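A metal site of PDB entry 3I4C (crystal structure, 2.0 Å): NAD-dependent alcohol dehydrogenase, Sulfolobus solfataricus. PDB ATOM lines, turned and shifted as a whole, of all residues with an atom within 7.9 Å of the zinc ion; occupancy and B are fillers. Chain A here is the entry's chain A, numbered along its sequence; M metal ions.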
ATOM      1  N   GLY A  36     -15.425   8.400 -26.208  1.00  0.00           N
ATOM      2  CA  GLY A  36     -14.278   8.084 -27.025  1.00  0.00           C
ATOM      3  C   GLY A  36     -13.948   6.600 -27.034  1.00  0.00           C
ATOM      4  O   GLY A  36     -14.242   5.883 -26.072  1.00  0.00           O
ATOM      5  N   VAL A  37     -13.357   6.156 -28.134  1.00  0.00           N
ATOM      6  CA  VAL A  37     -12.960   4.766 -28.308  1.00  0.00           C
ATOM      7  C   VAL A  37     -11.497   4.746 -28.720  1.00  0.00           C
ATOM      8  O   VAL A  37     -11.104   5.488 -29.612  1.00  0.00           O
ATOM      9  CB  VAL A  37     -13.784   4.067 -29.427  1.00  0.00           C
ATOM     10  CG1 VAL A  37     -13.334   2.620 -29.572  1.00  0.00           C
ATOM     11  CG2 VAL A  37     -15.265   4.147 -29.137  1.00  0.00           C
ATOM     12  N   CYS A  38     -10.693   3.911 -28.056  1.00  0.00           N
ATOM     13  CA  CYS A  38      -9.275   3.812 -28.421  1.00  0.00           C
ATOM     14  C   CYS A  38      -8.793   2.365 -28.383  1.00  0.00           C
ATOM     15  O   CYS A  38      -9.522   1.470 -27.973  1.00  0.00           O
ATOM     16  CB  CYS A  38      -8.408   4.682 -27.500  1.00  0.00           C
ATOM     17  SG  CYS A  38      -8.032   3.983 -25.873  1.00  0.00           S
ATOM     18  N   HIS A  39      -7.562   2.141 -28.834  1.00  0.00           N
ATOM     19  CA  HIS A  39      -6.996   0.797 -28.890  1.00  0.00           C
ATOM     20  C   HIS A  39      -7.118   0.029 -27.585  1.00  0.00           C
ATOM     21  O   HIS A  39      -7.166  -1.202 -27.579  1.00  0.00           O
ATOM     22  CB  HIS A  39      -5.531   0.849 -29.317  1.00  0.00           C
ATOM     23  CG  HIS A  39      -4.963  -0.486 -29.671  1.00  0.00           C
ATOM     24  ND1 HIS A  39      -5.466  -1.245 -30.712  1.00  0.00           N
ATOM     25  CD2 HIS A  39      -3.957  -1.206 -29.122  1.00  0.00           C
ATOM     26  CE1 HIS A  39      -4.786  -2.380 -30.786  1.00  0.00           C
ATOM     27  NE2 HIS A  39      -3.874  -2.380 -29.838  1.00  0.00           N
ATOM     28  N   SER A  40      -7.177   0.740 -26.456  1.00  0.00           N
ATOM     29  CA  SER A  40      -7.305   0.071 -25.172  1.00  0.00           C
ATOM     30  C   SER A  40      -8.593  -0.743 -25.099  1.00  0.00           C
ATOM     31  O   SER A  40      -8.655  -1.736 -24.372  1.00  0.00           O
ATOM     32  CB  SER A  40      -7.269   1.098 -24.033  1.00  0.00           C
ATOM     33  OG  SER A  40      -5.986   1.688 -23.917  1.00  0.00           O
ATOM     34  N   ASP A  41      -9.615  -0.317 -25.841  1.00  0.00           N
ATOM     35  CA  ASP A  41     -10.884  -1.032 -25.842  1.00  0.00           C
ATOM     36  C   ASP A  41     -10.767  -2.351 -26.601  1.00  0.00           C
ATOM     37  O   ASP A  41     -11.594  -3.259 -26.420  1.00  0.00           O
ATOM     38  CB  ASP A  41     -11.998  -0.173 -26.447  1.00  0.00           C
ATOM     39  CG  ASP A  41     -12.353   1.012 -25.560  1.00  0.00           C
ATOM     40  OD1 ASP A  41     -12.475   0.814 -24.338  1.00  0.00           O
ATOM     41  OD2 ASP A  41     -12.511   2.134 -26.086  1.00  0.00           O
ATOM     42  N   GLY A  67     -16.092   2.050 -22.143  1.00  0.00           N
ATOM     43  CA  GLY A  67     -16.122   3.491 -22.337  1.00  0.00           C
ATOM     44  C   GLY A  67     -15.438   4.250 -21.209  1.00  0.00           C
ATOM     45  O   GLY A  67     -16.088   4.663 -20.242  1.00  0.00           O
ATOM     46  N   HIS A  68     -14.136   4.446 -21.332  1.00  0.00           N
ATOM     47  CA  HIS A  68     -13.359   5.158 -20.317  1.00  0.00           C
ATOM     48  C   HIS A  68     -13.038   6.599 -20.719  1.00  0.00           C
ATOM     49  O   HIS A  68     -12.287   7.293 -20.026  1.00  0.00           O
ATOM     50  CB  HIS A  68     -12.062   4.420 -20.065  1.00  0.00           C
ATOM     51  CG  HIS A  68     -11.253   4.228 -21.308  1.00  0.00           C
ATOM     52  ND1 HIS A  68     -11.462   3.216 -22.217  1.00  0.00           N
ATOM     53  CD2 HIS A  68     -10.261   4.998 -21.828  1.00  0.00           C
ATOM     54  CE1 HIS A  68     -10.616   3.392 -23.239  1.00  0.00           C
ATOM     55  NE2 HIS A  68      -9.865   4.462 -23.043  1.00  0.00           N
ATOM     56  N   GLU A  69     -13.581   7.046 -21.856  1.00  0.00           N
ATOM     57  CA  GLU A  69     -13.362   8.410 -22.342  1.00  0.00           C
ATOM     58  C   GLU A  69     -14.737   9.076 -22.297  1.00  0.00           C
ATOM     59  O   GLU A  69     -15.514   9.020 -23.262  1.00  0.00           O
ATOM     60  CB  GLU A  69     -12.817   8.361 -23.765  1.00  0.00           C
ATOM     61  CG  GLU A  69     -11.472   7.641 -23.858  1.00  0.00           C
ATOM     62  CD  GLU A  69     -10.891   7.629 -25.269  1.00  0.00           C
ATOM     63  OE1 GLU A  69     -11.330   8.447 -26.096  1.00  0.00           O
ATOM     64  OE2 GLU A  69      -9.996   6.808 -25.552  1.00  0.00           O
ATOM     65  N   PRO A  94     -11.423   8.964 -15.523  1.00  0.00           N
ATOM     66  CA  PRO A  94     -11.898   7.600 -15.259  1.00  0.00           C
ATOM     67  C   PRO A  94     -11.125   6.710 -14.278  1.00  0.00           C
ATOM     68  O   PRO A  94     -11.672   5.713 -13.784  1.00  0.00           O
ATOM     69  CB  PRO A  94     -11.917   7.001 -16.651  1.00  0.00           C
ATOM     70  CG  PRO A  94     -10.655   7.574 -17.236  1.00  0.00           C
ATOM     71  CD  PRO A  94     -10.667   9.022 -16.783  1.00  0.00           C
ATOM     72  N   TRP A 117     -11.857   1.879 -12.219  1.00  0.00           N
ATOM     73  CA  TRP A 117     -11.590   2.416 -13.549  1.00  0.00           C
ATOM     74  C   TRP A 117     -12.833   2.372 -14.448  1.00  0.00           C
ATOM     75  O   TRP A 117     -13.171   1.310 -14.984  1.00  0.00           O
ATOM     76  CB  TRP A 117     -10.462   1.606 -14.170  1.00  0.00           C
ATOM     77  CG  TRP A 117      -9.744   2.251 -15.293  1.00  0.00           C
ATOM     78  CD1 TRP A 117     -10.165   3.311 -16.056  1.00  0.00           C
ATOM     79  CD2 TRP A 117      -8.457   1.874 -15.805  1.00  0.00           C
ATOM     80  NE1 TRP A 117      -9.219   3.614 -17.006  1.00  0.00           N
ATOM     81  CE2 TRP A 117      -8.160   2.752 -16.875  1.00  0.00           C
ATOM     82  CE3 TRP A 117      -7.532   0.886 -15.463  1.00  0.00           C
ATOM     83  CZ2 TRP A 117      -6.970   2.658 -17.601  1.00  0.00           C
ATOM     84  CZ3 TRP A 117      -6.350   0.795 -16.183  1.00  0.00           C
ATOM     85  CH2 TRP A 117      -6.077   1.673 -17.251  1.00  0.00           C
ATOM     86  N   ILE A 120     -13.528   0.120 -17.574  1.00  0.00           N
ATOM     87  CA  ILE A 120     -12.575  -0.988 -17.485  1.00  0.00           C
ATOM     88  C   ILE A 120     -13.076  -2.030 -16.487  1.00  0.00           C
ATOM     89  O   ILE A 120     -13.284  -3.186 -16.855  1.00  0.00           O
ATOM     90  CB  ILE A 120     -11.185  -0.488 -17.061  1.00  0.00           C
ATOM     91  CG1 ILE A 120     -10.706   0.595 -18.037  1.00  0.00           C
ATOM     92  CG2 ILE A 120     -10.192  -1.641 -17.017  1.00  0.00           C
ATOM     93  CD1 ILE A 120     -10.624   0.147 -19.471  1.00  0.00           C
ATOM     94  N   ALA A 150     -13.836  14.517 -24.650  1.00  0.00           N
ATOM     95  CA  ALA A 150     -13.751  13.094 -24.303  1.00  0.00           C
ATOM     96  C   ALA A 150     -12.385  12.446 -24.508  1.00  0.00           C
ATOM     97  O   ALA A 150     -11.869  11.788 -23.603  1.00  0.00           O
ATOM     98  CB  ALA A 150     -14.829  12.310 -25.061  1.00  0.00           C
ATOM     99  N   PRO A 151     -11.770  12.615 -25.681  1.00  0.00           N
ATOM    100  CA  PRO A 151     -10.462  12.003 -25.912  1.00  0.00           C
ATOM    101  C   PRO A 151      -9.358  12.514 -24.970  1.00  0.00           C
ATOM    102  O   PRO A 151      -8.370  11.825 -24.722  1.00  0.00           O
ATOM    103  CB  PRO A 151     -10.180  12.320 -27.376  1.00  0.00           C
ATOM    104  CG  PRO A 151     -11.570  12.415 -27.983  1.00  0.00           C
ATOM    105  CD  PRO A 151     -12.285  13.222 -26.927  1.00  0.00           C
ATOM    106  N   THR A 153      -9.503  12.872 -21.851  1.00  0.00           N
ATOM    107  CA  THR A 153      -9.529  12.143 -20.593  1.00  0.00           C
ATOM    108  C   THR A 153      -8.665  10.899 -20.663  1.00  0.00           C
ATOM    109  O   THR A 153      -8.438  10.244 -19.658  1.00  0.00           O
ATOM    110  CB  THR A 153     -10.938  11.680 -20.259  1.00  0.00           C
ATOM    111  OG1 THR A 153     -11.354  10.714 -21.242  1.00  0.00           O
ATOM    112  CG2 THR A 153     -11.900  12.855 -20.270  1.00  0.00           C
ATOM    113  N   CYS A 154      -8.177  10.576 -21.856  1.00  0.00           N
ATOM    114  CA  CYS A 154      -7.351   9.389 -22.039  1.00  0.00           C
ATOM    115  C   CYS A 154      -6.027   9.772 -22.693  1.00  0.00           C
ATOM    116  O   CYS A 154      -4.987   9.836 -22.022  1.00  0.00           O
ATOM    117  CB  CYS A 154      -8.108   8.374 -22.932  1.00  0.00           C
ATOM    118  SG  CYS A 154      -7.174   6.856 -23.334  1.00  0.00           S
ATOM    119  N   SER A 155      -6.074  10.074 -23.982  1.00  0.00           N
ATOM    120  CA  SER A 155      -4.865  10.451 -24.700  1.00  0.00           C
ATOM    121  C   SER A 155      -4.268  11.773 -24.187  1.00  0.00           C
ATOM    122  O   SER A 155      -3.058  11.946 -24.196  1.00  0.00           O
ATOM    123  CB  SER A 155      -5.174  10.544 -26.189  1.00  0.00           C
ATOM    124  OG  SER A 155      -5.576   9.266 -26.688  1.00  0.00           O
ATOM    125  N   THR A 158      -2.555  11.007 -20.765  1.00  0.00           N
ATOM    126  CA  THR A 158      -1.386  10.197 -21.070  1.00  0.00           C
ATOM    127  C   THR A 158      -0.235  11.018 -21.628  1.00  0.00           C
ATOM    128  O   THR A 158       0.896  10.943 -21.117  1.00  0.00           O
ATOM    129  CB  THR A 158      -1.729   9.099 -22.100  1.00  0.00           C
ATOM    130  OG1 THR A 158      -2.593   8.129 -21.503  1.00  0.00           O
ATOM    131  CG2 THR A 158      -0.449   8.410 -22.592  1.00  0.00           C
ATOM    132  N   ARG A 342      -9.506   9.624 -34.097  1.00  0.00           N
ATOM    133  CA  ARG A 342     -10.208   9.259 -32.876  1.00  0.00           C
ATOM    134  C   ARG A 342     -11.712   9.125 -33.072  1.00  0.00           C
ATOM    135  O   ARG A 342     -12.399  10.088 -33.397  1.00  0.00           O
ATOM    136  CB  ARG A 342      -9.900  10.277 -31.768  1.00  0.00           C
ATOM    137  CG  ARG A 342     -10.554   9.975 -30.427  1.00  0.00           C
ATOM    138  CD  ARG A 342     -10.238   8.571 -29.935  1.00  0.00           C
ATOM    139  NE  ARG A 342      -8.797   8.338 -29.855  1.00  0.00           N
ATOM    140  CZ  ARG A 342      -8.080   8.379 -28.738  1.00  0.00           C
ATOM    141  NH1 ARG A 342      -8.650   8.636 -27.571  1.00  0.00           N
ATOM    142  NH2 ARG A 342      -6.779   8.159 -28.800  1.00  0.00           N
HETATM  143 ZN    ZN M   1      -8.779   5.566 -24.399  1.00  0.00          ZN
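A ring nitrogen (ND1) of His 68 lies within hydrogen-bond range of the side-chain carboxylate of Asp 41, 3.4 Å away. The guanidinium group (NH1) of Arg 342 lies within salt-bridge range of the side-chain carboxylate (OE1) of Glu 69 (3.1 Å). The backbone carbonyl oxygen (O) of Glu 69 is in hydrogen-bond range of the backbone NH (N) of Gly 36 (3.0 Å). SG of Cys 38 lies close to N of Ser 40 (3.4 Å). The backbone NH of Cys 38 sits at hydrogen-bond distance from the side-chain carboxylate of Asp 41 (3.2 Å). O of Cys 154 sits at hydrogen-bond distance from OG1 of Thr 158 (3.0 Å).
The nearest printed residue that does not touch the zinc ion is Arg 342 (4.4 Å).
The zinc ion is bound by NE2 of His 68, OE2 of Glu 69, SG of Cys 38 and SG of Cys 154.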
